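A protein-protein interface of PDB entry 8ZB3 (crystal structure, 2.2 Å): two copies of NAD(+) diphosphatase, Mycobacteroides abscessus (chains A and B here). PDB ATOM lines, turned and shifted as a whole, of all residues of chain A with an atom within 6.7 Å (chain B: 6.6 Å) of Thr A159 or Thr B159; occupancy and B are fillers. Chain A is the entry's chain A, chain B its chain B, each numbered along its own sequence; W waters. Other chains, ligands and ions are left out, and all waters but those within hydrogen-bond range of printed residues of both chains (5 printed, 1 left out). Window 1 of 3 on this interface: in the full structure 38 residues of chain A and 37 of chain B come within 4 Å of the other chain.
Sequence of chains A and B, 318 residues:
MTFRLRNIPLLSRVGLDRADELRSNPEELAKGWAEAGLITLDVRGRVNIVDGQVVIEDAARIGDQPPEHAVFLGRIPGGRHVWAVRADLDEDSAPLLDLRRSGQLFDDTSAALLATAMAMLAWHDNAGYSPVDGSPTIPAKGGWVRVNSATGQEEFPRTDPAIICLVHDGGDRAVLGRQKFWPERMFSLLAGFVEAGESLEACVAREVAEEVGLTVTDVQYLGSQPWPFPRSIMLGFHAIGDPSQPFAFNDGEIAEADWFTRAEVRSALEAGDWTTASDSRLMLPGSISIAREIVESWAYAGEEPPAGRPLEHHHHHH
The guanidinium group (NH2) of Arg A158 sits at hydrogen-bond distance from the backbone carbonyl oxygen (O) of Phe B156 (2.9 Å). The backbone carbonyl oxygen (O) of Phe A156 lies within hydrogen-bond range of the guanidinium group (NH2) of Arg B158, 3.0 Å away. NH2 of Arg A158 lies within hydrogen-bond range of O of Pro B157 (3.3 Å). The backbone carbonyl oxygen (O) of Pro A157 is in hydrogen-bond range of the guanidinium group (NH2) of Arg B158 (3.3 Å).
The backbone carbonyl oxygen (O) of Pro A161 sits at hydrogen-bond distance from the backbone NH (N) of Val A194 (3.0 Å). O of Pro B161 is in hydrogen-bond range of N of Val B194. The backbone NH (N) of Glu A195 lies within hydrogen-bond range of the side-chain carboxylate (OE2) of Glu A198 (2.8 Å). O of Asp B160 sits at hydrogen-bond distance from N of Ile B233 (3.0 Å). NE of Arg B158 lies within salt-bridge range of OD1 of Asp B160. The backbone NH of Glu B195 lies within hydrogen-bond range of the side-chain carboxylate of Glu B198 (2.8 Å).
Among the printed residues, pairs that only touch across the chains: Ala A119 with Ala B196 (3.6 Å), Arg A158 with Arg B158 (3.4 Å), Thr A159 with Thr B159 (3.95 Å), Thr A159 with Pro B161 (3.4 Å), Thr A159 with Ala B196 (3.9 Å), Pro A161 with Thr B159 (3.3 Å), Pro A161 with Pro B161 (3.99 Å), Ala A196 with Ala B119 (3.4 Å), Ala A196 with Thr B159 (3.7 Å), Gly A197 with Ala B119 (3.9 Å), Gly A197 with Pro B226 (3.6 Å), Glu A198 with Pro B226 (3.8 Å), Glu A198 with Ile B233 (3.5 Å), Pro A226 with Gly B197 (3.6 Å), Pro A226 with Glu B198 (3.9 Å) and Ile A233 with Glu B198 (3.5 Å).
Of chain B, only Thr B159 (3.95 Å), Pro B161 (3.4 Å) and Ala B196 (3.9 Å) come within 4 Å of Thr A159. Printed residues of chain B within 4 Å of Ala A196: Ala B119 (3.4 Å) and Thr B159 (3.7 Å). Of the printed residues of chain A, Thr B159 touches Thr A159, Pro A161 and Ala A196. Glu B195 touches none of the printed residues of chain A. Of the printed residues of chain A, Ala B196 touches Ala A119 and Thr A159. Printed residues of chain A within 4 Å of Glu B198: Pro A226 and Ile A233. The nearest residue of chain A that does not touch Thr B159 is Glu A195 (4.2 Å). The nearest printed residue of chain B that does not touch Ala A119 is Gly B197 (4.7 Å).
Printed residues of chain B that touch a printed residue of chain A: Ala B119, Phe B156, Pro B157, Arg B158, Thr B159, Pro B161, Ala B196, Gly B197, Glu B198, Pro B226 and Ile B233. Hydrophobic or aromatic side chains of chain B within 4 Å of the printed part of chain A: Ala B119, Pro B161, Ala B196, Pro B226 and Ile B233. Among the printed residues, 20 pairs touch across the chains. Among the printed residues, no Asp or Glu carboxylate lies within 4 Å of a Lys or Arg side-chain nitrogen of the other chain.
Pro A157 touches Arg B158, and with the chains exchanged Arg A158 touches Pro B157. Gly A197 touches Pro B226, and with the chains exchanged Pro A226 touches Gly B197. Glu A198 touches Pro B226, and with the chains exchanged Pro A226 touches Glu B198. Glu A198 touches Ile B233, and with the chains exchanged Ile A233 touches Glu B198. Positions printed for both chains: 119, 156, 157, 158, 159, 160, 161, 194, 195, 196, 197, 198, 226, 227, 231, 232 and 233.
Water W2 lies within hydrogen-bond range of OG1 of Thr A159, O of Val B194 and O of Pro A157. Water W3 lies within hydrogen-bond range of the backbone NH of Phe B156 and the guanidinium group of Arg A231. Water W1 lies within hydrogen-bond range of OG1 of Thr B159, O of Pro B157 and O of Val A194. Water W4 bridges the guanidinium group (NH2) of Arg B231 (2.8 Å) and the backbone NH (N) of Phe A156 (3.0 Å). Water W5 lies within hydrogen-bond range of N of Thr B159 (3.0 Å), OD1 of Asp A160 (3.2 Å) and O of Pro B157 (3.3 Å).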
ATOM      1  N   ALA A 119      10.862 -11.430 -25.080  1.00  0.00           N
ATOM      2  CA  ALA A 119       9.907 -12.239 -25.818  1.00  0.00           C
ATOM      3  C   ALA A 119      10.200 -12.179 -27.317  1.00  0.00           C
ATOM      4  O   ALA A 119      10.203 -13.198 -27.999  1.00  0.00           O
ATOM      5  CB  ALA A 119       8.496 -11.758 -25.523  1.00  0.00           C
ATOM      6  N   PHE A 156       4.107 -14.192 -37.496  1.00  0.00           N
ATOM      7  CA  PHE A 156       3.905 -13.217 -36.426  1.00  0.00           C
ATOM      8  C   PHE A 156       4.400 -13.761 -35.083  1.00  0.00           C
ATOM      9  O   PHE A 156       4.406 -14.967 -34.846  1.00  0.00           O
ATOM     10  CB  PHE A 156       2.426 -12.859 -36.337  1.00  0.00           C
ATOM     11  CG  PHE A 156       1.897 -12.248 -37.609  1.00  0.00           C
ATOM     12  CD1 PHE A 156       2.164 -10.925 -37.945  1.00  0.00           C
ATOM     13  CD2 PHE A 156       1.163 -13.007 -38.500  1.00  0.00           C
ATOM     14  CE1 PHE A 156       1.680 -10.377 -39.124  1.00  0.00           C
ATOM     15  CE2 PHE A 156       0.698 -12.461 -39.690  1.00  0.00           C
ATOM     16  CZ  PHE A 156       0.971 -11.148 -40.003  1.00  0.00           C
ATOM     17  N   PRO A 157       4.837 -12.888 -34.154  1.00  0.00           N
ATOM     18  CA  PRO A 157       5.306 -13.329 -32.839  1.00  0.00           C
ATOM     19  C   PRO A 157       4.275 -14.168 -32.107  1.00  0.00           C
ATOM     20  O   PRO A 157       3.088 -13.882 -32.147  1.00  0.00           O
ATOM     21  CB  PRO A 157       5.489 -12.016 -32.078  1.00  0.00           C
ATOM     22  CG  PRO A 157       5.815 -11.021 -33.161  1.00  0.00           C
ATOM     23  CD  PRO A 157       4.929 -11.426 -34.322  1.00  0.00           C
ATOM     24  N   ARG A 158       4.757 -15.215 -31.436  1.00  0.00           N
ATOM     25  CA  ARG A 158       3.866 -16.134 -30.758  1.00  0.00           C
ATOM     26  C   ARG A 158       3.853 -15.879 -29.253  1.00  0.00           C
ATOM     27  O   ARG A 158       4.905 -15.812 -28.621  1.00  0.00           O
ATOM     28  CB  ARG A 158       4.355 -17.558 -31.028  1.00  0.00           C
ATOM     29  CG  ARG A 158       3.509 -18.609 -30.327  1.00  0.00           C
ATOM     30  CD  ARG A 158       4.036 -19.960 -30.760  1.00  0.00           C
ATOM     31  NE  ARG A 158       3.293 -21.019 -30.116  1.00  0.00           N
ATOM     32  CZ  ARG A 158       3.204 -22.249 -30.572  1.00  0.00           C
ATOM     33  NH1 ARG A 158       3.845 -22.593 -31.678  1.00  0.00           N
ATOM     34  NH2 ARG A 158       2.433 -23.103 -29.942  1.00  0.00           N
ATOM     35  N   THR A 159       2.645 -15.798 -28.698  1.00  0.00           N
ATOM     36  CA  THR A 159       2.427 -15.710 -27.267  1.00  0.00           C
ATOM     37  C   THR A 159       1.390 -16.767 -26.896  1.00  0.00           C
ATOM     38  O   THR A 159       0.255 -16.691 -27.346  1.00  0.00           O
ATOM     39  CB  THR A 159       1.968 -14.300 -26.871  1.00  0.00           C
ATOM     40  OG1 THR A 159       2.946 -13.386 -27.366  1.00  0.00           O
ATOM     41  CG2 THR A 159       1.730 -14.130 -25.376  1.00  0.00           C
ATOM     42  N   ASP A 160       1.796 -17.753 -26.093  1.00  0.00           N
ATOM     43  CA  ASP A 160       0.943 -18.851 -25.702  1.00  0.00           C
ATOM     44  C   ASP A 160       0.169 -18.457 -24.443  1.00  0.00           C
ATOM     45  O   ASP A 160       0.756 -18.163 -23.402  1.00  0.00           O
ATOM     46  CB  ASP A 160       1.776 -20.089 -25.388  1.00  0.00           C
ATOM     47  CG  ASP A 160       2.527 -20.684 -26.553  1.00  0.00           C
ATOM     48  OD1 ASP A 160       2.116 -20.457 -27.690  1.00  0.00           O
ATOM     49  OD2 ASP A 160       3.510 -21.382 -26.307  1.00  0.00           O
ATOM     50  N   PRO A 161      -1.177 -18.434 -24.474  1.00  0.00           N
ATOM     51  CA  PRO A 161      -1.945 -18.177 -23.265  1.00  0.00           C
ATOM     52  C   PRO A 161      -1.896 -19.362 -22.306  1.00  0.00           C
ATOM     53  O   PRO A 161      -2.009 -20.508 -22.717  1.00  0.00           O
ATOM     54  CB  PRO A 161      -3.347 -17.866 -23.792  1.00  0.00           C
ATOM     55  CG  PRO A 161      -3.417 -18.493 -25.129  1.00  0.00           C
ATOM     56  CD  PRO A 161      -2.004 -18.593 -25.660  1.00  0.00           C
ATOM     57  N   VAL A 194      -3.560 -23.071 -22.449  1.00  0.00           N
ATOM     58  CA  VAL A 194      -4.823 -23.165 -23.153  1.00  0.00           C
ATOM     59  C   VAL A 194      -4.613 -24.023 -24.385  1.00  0.00           C
ATOM     60  O   VAL A 194      -3.707 -23.757 -25.170  1.00  0.00           O
ATOM     61  CB  VAL A 194      -5.355 -21.775 -23.546  1.00  0.00           C
ATOM     62  CG1 VAL A 194      -6.656 -21.910 -24.314  1.00  0.00           C
ATOM     63  CG2 VAL A 194      -5.542 -20.876 -22.334  1.00  0.00           C
ATOM     64  N   GLU A 195      -5.503 -25.007 -24.585  1.00  0.00           N
ATOM     65  CA  GLU A 195      -5.426 -25.864 -25.766  1.00  0.00           C
ATOM     66  C   GLU A 195      -6.361 -25.326 -26.844  1.00  0.00           C
ATOM     67  O   GLU A 195      -7.268 -24.525 -26.579  1.00  0.00           O
ATOM     68  CB  GLU A 195      -5.816 -27.296 -25.421  1.00  0.00           C
ATOM     69  CG  GLU A 195      -4.856 -27.964 -24.456  1.00  0.00           C
ATOM     70  CD  GLU A 195      -5.040 -29.461 -24.248  1.00  0.00           C
ATOM     71  OE1 GLU A 195      -4.198 -30.024 -23.546  1.00  0.00           O
ATOM     72  OE2 GLU A 195      -6.072 -30.037 -24.699  1.00  0.00           O
ATOM     73  N   ALA A 196      -6.104 -25.768 -28.074  1.00  0.00           N
ATOM     74  CA  ALA A 196      -6.957 -25.493 -29.214  1.00  0.00           C
ATOM     75  C   ALA A 196      -8.385 -25.938 -28.922  1.00  0.00           C
ATOM     76  O   ALA A 196      -8.605 -27.040 -28.402  1.00  0.00           O
ATOM     77  CB  ALA A 196      -6.429 -26.241 -30.416  1.00  0.00           C
ATOM     78  N   GLY A 197      -9.350 -25.087 -29.276  1.00  0.00           N
ATOM     79  CA  GLY A 197     -10.739 -25.509 -29.291  1.00  0.00           C
ATOM     80  C   GLY A 197     -11.441 -25.342 -27.944  1.00  0.00           C
ATOM     81  O   GLY A 197     -12.587 -25.774 -27.797  1.00  0.00           O
ATOM     82  N   GLU A 198     -10.784 -24.713 -26.955  1.00  0.00           N
ATOM     83  CA  GLU A 198     -11.452 -24.507 -25.679  1.00  0.00           C
ATOM     84  C   GLU A 198     -11.438 -23.029 -25.288  1.00  0.00           C
ATOM     85  O   GLU A 198     -10.545 -22.264 -25.668  1.00  0.00           O
ATOM     86  CB  GLU A 198     -10.828 -25.381 -24.586  1.00  0.00           C
ATOM     87  CG  GLU A 198      -9.410 -24.986 -24.203  1.00  0.00           C
ATOM     88  CD  GLU A 198      -8.770 -25.883 -23.148  1.00  0.00           C
ATOM     89  OE1 GLU A 198      -9.466 -26.799 -22.655  1.00  0.00           O
ATOM     90  OE2 GLU A 198      -7.572 -25.644 -22.787  1.00  0.00           O
ATOM     91  N   PRO A 226       2.230 -10.593 -18.833  1.00  0.00           N
ATOM     92  CA  PRO A 226       3.192 -11.158 -19.781  1.00  0.00           C
ATOM     93  C   PRO A 226       4.189 -12.021 -19.027  1.00  0.00           C
ATOM     94  O   PRO A 226       4.557 -11.705 -17.907  1.00  0.00           O
ATOM     95  CB  PRO A 226       3.882  -9.956 -20.453  1.00  0.00           C
ATOM     96  CG  PRO A 226       3.470  -8.748 -19.650  1.00  0.00           C
ATOM     97  CD  PRO A 226       2.259  -9.129 -18.801  1.00  0.00           C
ATOM     98  N   TRP A 227       4.600 -13.125 -19.646  1.00  0.00           N
ATOM     99  CA  TRP A 227       5.421 -14.109 -18.962  1.00  0.00           C
ATOM    100  C   TRP A 227       6.404 -14.700 -19.967  1.00  0.00           C
ATOM    101  O   TRP A 227       6.284 -15.847 -20.388  1.00  0.00           O
ATOM    102  CB  TRP A 227       4.534 -15.166 -18.306  1.00  0.00           C
ATOM    103  CG  TRP A 227       5.244 -15.929 -17.226  1.00  0.00           C
ATOM    104  CD1 TRP A 227       5.586 -17.246 -17.246  1.00  0.00           C
ATOM    105  CD2 TRP A 227       5.729 -15.398 -15.979  1.00  0.00           C
ATOM    106  NE1 TRP A 227       6.247 -17.567 -16.093  1.00  0.00           N
ATOM    107  CE2 TRP A 227       6.354 -16.467 -15.297  1.00  0.00           C
ATOM    108  CE3 TRP A 227       5.713 -14.130 -15.376  1.00  0.00           C
ATOM    109  CZ2 TRP A 227       6.946 -16.306 -14.044  1.00  0.00           C
ATOM    110  CZ3 TRP A 227       6.308 -13.968 -14.138  1.00  0.00           C
ATOM    111  CH2 TRP A 227       6.908 -15.044 -13.480  1.00  0.00           C
ATOM    112  N   ARG A 231       7.621 -17.534 -23.732  1.00  0.00           N
ATOM    113  CA  ARG A 231       6.626 -16.930 -24.610  1.00  0.00           C
ATOM    114  C   ARG A 231       5.186 -17.066 -24.123  1.00  0.00           C
ATOM    115  O   ARG A 231       4.288 -17.198 -24.934  1.00  0.00           O
ATOM    116  CB  ARG A 231       6.770 -17.569 -25.991  1.00  0.00           C
ATOM    117  CG  ARG A 231       6.350 -19.025 -26.056  1.00  0.00           C
ATOM    118  CD  ARG A 231       6.553 -19.595 -27.438  1.00  0.00           C
ATOM    119  NE  ARG A 231       5.904 -20.894 -27.539  1.00  0.00           N
ATOM    120  CZ  ARG A 231       6.206 -21.822 -28.436  1.00  0.00           C
ATOM    121  NH1 ARG A 231       7.124 -21.591 -29.356  1.00  0.00           N
ATOM    122  NH2 ARG A 231       5.576 -22.986 -28.399  1.00  0.00           N
ATOM    123  N   SER A 232       4.927 -16.921 -22.828  1.00  0.00           N
ATOM    124  CA  SER A 232       3.571 -17.049 -22.325  1.00  0.00           C
ATOM    125  C   SER A 232       2.949 -15.689 -22.045  1.00  0.00           C
ATOM    126  O   SER A 232       3.643 -14.683 -21.903  1.00  0.00           O
ATOM    127  CB  SER A 232       3.554 -17.886 -21.064  1.00  0.00           C
ATOM    128  OG  SER A 232       4.017 -19.186 -21.335  1.00  0.00           O
ATOM    129  N   ILE A 233       1.621 -15.704 -21.901  1.00  0.00           N
ATOM    130  CA  ILE A 233       0.910 -14.703 -21.128  1.00  0.00           C
ATOM    131  C   ILE A 233       0.094 -15.470 -20.089  1.00  0.00           C
ATOM    132  O   ILE A 233      -0.630 -16.397 -20.425  1.00  0.00           O
ATOM    133  CB  ILE A 233       0.045 -13.778 -22.012  1.00  0.00           C
ATOM    134  CG1 ILE A 233      -0.670 -12.739 -21.151  1.00  0.00           C
ATOM    135  CG2 ILE A 233      -0.944 -14.554 -22.868  1.00  0.00           C
ATOM    136  CD1 ILE A 233      -1.390 -11.667 -21.927  1.00  0.00           C
ATOM    137  N   ALA B 119      -9.460 -26.609 -35.003  1.00  0.00           N
ATOM    138  CA  ALA B 119      -8.250 -25.946 -34.524  1.00  0.00           C
ATOM    139  C   ALA B 119      -7.037 -26.865 -34.661  1.00  0.00           C
ATOM    140  O   ALA B 119      -5.981 -26.450 -35.148  1.00  0.00           O
ATOM    141  CB  ALA B 119      -8.470 -25.533 -33.087  1.00  0.00           C
ATOM    142  N   PHE B 156       4.079 -27.607 -30.141  1.00  0.00           N
ATOM    143  CA  PHE B 156       2.773 -27.668 -29.498  1.00  0.00           C
ATOM    144  C   PHE B 156       1.746 -26.835 -30.258  1.00  0.00           C
ATOM    145  O   PHE B 156       2.087 -25.852 -30.910  1.00  0.00           O
ATOM    146  CB  PHE B 156       2.868 -27.187 -28.054  1.00  0.00           C
ATOM    147  CG  PHE B 156       3.836 -27.994 -27.227  1.00  0.00           C
ATOM    148  CD1 PHE B 156       3.474 -29.233 -26.729  1.00  0.00           C
ATOM    149  CD2 PHE B 156       5.125 -27.532 -26.993  1.00  0.00           C
ATOM    150  CE1 PHE B 156       4.379 -29.996 -26.012  1.00  0.00           C
ATOM    151  CE2 PHE B 156       6.023 -28.292 -26.265  1.00  0.00           C
ATOM    152  CZ  PHE B 156       5.652 -29.535 -25.802  1.00  0.00           C
ATOM    153  N   PRO B 157       0.444 -27.197 -30.200  1.00  0.00           N
ATOM    154  CA  PRO B 157      -0.596 -26.442 -30.881  1.00  0.00           C
ATOM    155  C   PRO B 157      -0.606 -24.962 -30.519  1.00  0.00           C
ATOM    156  O   PRO B 157      -0.435 -24.602 -29.378  1.00  0.00           O
ATOM    157  CB  PRO B 157      -1.889 -27.091 -30.382  1.00  0.00           C
ATOM    158  CG  PRO B 157      -1.495 -28.493 -30.084  1.00  0.00           C
ATOM    159  CD  PRO B 157      -0.102 -28.363 -29.494  1.00  0.00           C
ATOM    160  N   ARG B 158      -0.842 -24.125 -31.514  1.00  0.00           N
ATOM    161  CA  ARG B 158      -0.783 -22.688 -31.344  1.00  0.00           C
ATOM    162  C   ARG B 158      -2.185 -22.096 -31.319  1.00  0.00           C
ATOM    163  O   ARG B 158      -2.972 -22.334 -32.236  1.00  0.00           O
ATOM    164  CB  ARG B 158      -0.001 -22.069 -32.504  1.00  0.00           C
ATOM    165  CG  ARG B 158       0.116 -20.568 -32.367  1.00  0.00           C
ATOM    166  CD  ARG B 158       1.018 -20.060 -33.450  1.00  0.00           C
ATOM    167  NE  ARG B 158       1.126 -18.620 -33.383  1.00  0.00           N
ATOM    168  CZ  ARG B 158       2.127 -17.929 -33.878  1.00  0.00           C
ATOM    169  NH1 ARG B 158       3.096 -18.540 -34.538  1.00  0.00           N
ATOM    170  NH2 ARG B 158       2.166 -16.624 -33.687  1.00  0.00           N
ATOM    171  N   THR B 159      -2.452 -21.290 -30.289  1.00  0.00           N
ATOM    172  CA  THR B 159      -3.683 -20.525 -30.187  1.00  0.00           C
ATOM    173  C   THR B 159      -3.321 -19.079 -29.869  1.00  0.00           C
ATOM    174  O   THR B 159      -2.743 -18.799 -28.831  1.00  0.00           O
ATOM    175  CB  THR B 159      -4.596 -21.129 -29.109  1.00  0.00           C
ATOM    176  OG1 THR B 159      -4.845 -22.482 -29.492  1.00  0.00           O
ATOM    177  CG2 THR B 159      -5.922 -20.406 -28.965  1.00  0.00           C
ATOM    178  N   ASP B 160      -3.633 -18.165 -30.793  1.00  0.00           N
ATOM    179  CA  ASP B 160      -3.281 -16.763 -30.668  1.00  0.00           C
ATOM    180  C   ASP B 160      -4.387 -16.034 -29.911  1.00  0.00           C
ATOM    181  O   ASP B 160      -5.540 -16.050 -30.317  1.00  0.00           O
ATOM    182  CB  ASP B 160      -3.119 -16.132 -32.046  1.00  0.00           C
ATOM    183  CG  ASP B 160      -1.941 -16.661 -32.858  1.00  0.00           C
ATOM    184  OD1 ASP B 160      -1.009 -17.227 -32.287  1.00  0.00           O
ATOM    185  OD2 ASP B 160      -1.993 -16.504 -34.077  1.00  0.00           O
ATOM    186  N   PRO B 161      -4.098 -15.408 -28.758  1.00  0.00           N
ATOM    187  CA  PRO B 161      -5.121 -14.653 -28.039  1.00  0.00           C
ATOM    188  C   PRO B 161      -5.418 -13.333 -28.753  1.00  0.00           C
ATOM    189  O   PRO B 161      -4.508 -12.633 -29.174  1.00  0.00           O
ATOM    190  CB  PRO B 161      -4.538 -14.454 -26.641  1.00  0.00           C
ATOM    191  CG  PRO B 161      -3.073 -14.660 -26.782  1.00  0.00           C
ATOM    192  CD  PRO B 161      -2.835 -15.495 -28.032  1.00  0.00           C
ATOM    193  N   VAL B 194      -3.108  -9.953 -29.179  1.00  0.00           N
ATOM    194  CA  VAL B 194      -2.190  -9.637 -28.094  1.00  0.00           C
ATOM    195  C   VAL B 194      -0.744  -9.680 -28.596  1.00  0.00           C
ATOM    196  O   VAL B 194      -0.334 -10.639 -29.214  1.00  0.00           O
ATOM    197  CB  VAL B 194      -2.368 -10.610 -26.914  1.00  0.00           C
ATOM    198  CG1 VAL B 194      -1.386 -10.309 -25.799  1.00  0.00           C
ATOM    199  CG2 VAL B 194      -3.777 -10.560 -26.353  1.00  0.00           C
ATOM    200  N   GLU B 195       0.049  -8.662 -28.265  1.00  0.00           N
ATOM    201  CA  GLU B 195       1.464  -8.641 -28.605  1.00  0.00           C
ATOM    202  C   GLU B 195       2.301  -9.128 -27.421  1.00  0.00           C
ATOM    203  O   GLU B 195       1.852  -9.150 -26.280  1.00  0.00           O
ATOM    204  CB  GLU B 195       1.935  -7.235 -28.984  1.00  0.00           C
ATOM    205  CG  GLU B 195       1.298  -6.699 -30.239  1.00  0.00           C
ATOM    206  CD  GLU B 195       1.935  -5.405 -30.767  1.00  0.00           C
ATOM    207  OE1 GLU B 195       1.520  -4.949 -31.814  1.00  0.00           O
ATOM    208  OE2 GLU B 195       2.968  -4.919 -30.205  1.00  0.00           O
ATOM    209  N   ALA B 196       3.542  -9.506 -27.734  1.00  0.00           N
ATOM    210  CA  ALA B 196       4.530  -9.874 -26.750  1.00  0.00           C
ATOM    211  C   ALA B 196       4.762  -8.708 -25.796  1.00  0.00           C
ATOM    212  O   ALA B 196       4.884  -7.562 -26.205  1.00  0.00           O
ATOM    213  CB  ALA B 196       5.820 -10.242 -27.458  1.00  0.00           C
ATOM    214  N   GLY B 197       4.849  -9.007 -24.511  1.00  0.00           N
ATOM    215  CA  GLY B 197       5.260  -8.033 -23.523  1.00  0.00           C
ATOM    216  C   GLY B 197       4.111  -7.215 -22.959  1.00  0.00           C
ATOM    217  O   GLY B 197       4.371  -6.287 -22.186  1.00  0.00           O
ATOM    218  N   GLU B 198       2.859  -7.530 -23.314  1.00  0.00           N
ATOM    219  CA  GLU B 198       1.756  -6.713 -22.802  1.00  0.00           C
ATOM    220  C   GLU B 198       0.708  -7.582 -22.103  1.00  0.00           C
ATOM    221  O   GLU B 198       0.535  -8.757 -22.445  1.00  0.00           O
ATOM    222  CB  GLU B 198       1.120  -5.845 -23.898  1.00  0.00           C
ATOM    223  CG  GLU B 198       0.334  -6.617 -24.933  1.00  0.00           C
ATOM    224  CD  GLU B 198      -0.286  -5.761 -26.037  1.00  0.00           C
ATOM    225  OE1 GLU B 198      -0.180  -4.511 -25.951  1.00  0.00           O
ATOM    226  OE2 GLU B 198      -0.903  -6.346 -26.989  1.00  0.00           O
ATOM    227  N   PRO B 226     -13.278 -20.048 -28.197  1.00  0.00           N
ATOM    228  CA  PRO B 226     -12.379 -20.553 -29.216  1.00  0.00           C
ATOM    229  C   PRO B 226     -12.826 -20.013 -30.565  1.00  0.00           C
ATOM    230  O   PRO B 226     -14.014 -19.882 -30.821  1.00  0.00           O
ATOM    231  CB  PRO B 226     -12.483 -22.082 -29.150  1.00  0.00           C
ATOM    232  CG  PRO B 226     -13.656 -22.367 -28.249  1.00  0.00           C
ATOM    233  CD  PRO B 226     -13.968 -21.112 -27.465  1.00  0.00           C
ATOM    234  N   TRP B 227     -11.858 -19.700 -31.422  1.00  0.00           N
ATOM    235  CA  TRP B 227     -12.155 -19.048 -32.678  1.00  0.00           C
ATOM    236  C   TRP B 227     -11.200 -19.579 -33.733  1.00  0.00           C
ATOM    237  O   TRP B 227     -10.286 -18.889 -34.172  1.00  0.00           O
ATOM    238  CB  TRP B 227     -12.065 -17.530 -32.506  1.00  0.00           C
ATOM    239  CG  TRP B 227     -12.782 -16.771 -33.582  1.00  0.00           C
ATOM    240  CD1 TRP B 227     -12.225 -15.985 -34.545  1.00  0.00           C
ATOM    241  CD2 TRP B 227     -14.204 -16.767 -33.809  1.00  0.00           C
ATOM    242  NE1 TRP B 227     -13.206 -15.476 -35.340  1.00  0.00           N
ATOM    243  CE2 TRP B 227     -14.424 -15.940 -34.930  1.00  0.00           C
ATOM    244  CE3 TRP B 227     -15.307 -17.378 -33.190  1.00  0.00           C
ATOM    245  CZ2 TRP B 227     -15.699 -15.716 -35.449  1.00  0.00           C
ATOM    246  CZ3 TRP B 227     -16.565 -17.166 -33.710  1.00  0.00           C
ATOM    247  CH2 TRP B 227     -16.757 -16.337 -34.821  1.00  0.00           C
ATOM    248  N   ARG B 231      -6.857 -19.917 -35.892  1.00  0.00           N
ATOM    249  CA  ARG B 231      -6.200 -20.328 -34.663  1.00  0.00           C
ATOM    250  C   ARG B 231      -6.284 -19.298 -33.534  1.00  0.00           C
ATOM    251  O   ARG B 231      -5.348 -19.171 -32.758  1.00  0.00           O
ATOM    252  CB  ARG B 231      -4.728 -20.625 -34.974  1.00  0.00           C
ATOM    253  CG  ARG B 231      -3.907 -19.394 -35.353  1.00  0.00           C
ATOM    254  CD  ARG B 231      -2.482 -19.791 -35.687  1.00  0.00           C
ATOM    255  NE  ARG B 231      -1.649 -18.612 -35.787  1.00  0.00           N
ATOM    256  CZ  ARG B 231      -0.499 -18.532 -36.445  1.00  0.00           C
ATOM    257  NH1 ARG B 231       0.004 -19.577 -37.071  1.00  0.00           N
ATOM    258  NH2 ARG B 231       0.156 -17.388 -36.477  1.00  0.00           N
ATOM    259  N   SER B 232      -7.425 -18.644 -33.348  1.00  0.00           N
ATOM    260  CA  SER B 232      -7.544 -17.656 -32.288  1.00  0.00           C
ATOM    261  C   SER B 232      -8.301 -18.215 -31.087  1.00  0.00           C
ATOM    262  O   SER B 232      -9.027 -19.199 -31.186  1.00  0.00           O
ATOM    263  CB  SER B 232      -8.232 -16.416 -32.794  1.00  0.00           C
ATOM    264  OG  SER B 232      -7.447 -15.821 -33.782  1.00  0.00           O
ATOM    265  N   ILE B 233      -8.146 -17.524 -29.961  1.00  0.00           N
ATOM    266  CA  ILE B 233      -9.139 -17.527 -28.898  1.00  0.00           C
ATOM    267  C   ILE B 233      -9.529 -16.072 -28.673  1.00  0.00           C
ATOM    268  O   ILE B 233      -8.668 -15.214 -28.526  1.00  0.00           O
ATOM    269  CB  ILE B 233      -8.627 -18.211 -27.606  1.00  0.00           C
ATOM    270  CG1 ILE B 233      -9.714 -18.210 -26.532  1.00  0.00           C
ATOM    271  CG2 ILE B 233      -7.342 -17.582 -27.086  1.00  0.00           C
ATOM    272  CD1 ILE B 233      -9.363 -18.983 -25.285  1.00  0.00           C
HETATM  273  O   HOH W   1      -3.018 -24.073 -28.066  1.00  0.00           O
HETATM  274  O   HOH W   2       2.094 -12.231 -29.684  1.00  0.00           O
HETATM  275  O   HOH W   3       5.606 -25.338 -30.013  1.00  0.00           O
HETATM  276  O   HOH W   4       2.482 -16.711 -37.905  1.00  0.00           O
HETATM  277  O   HOH W   5      -0.782 -21.700 -27.826  1.00  0.00           O
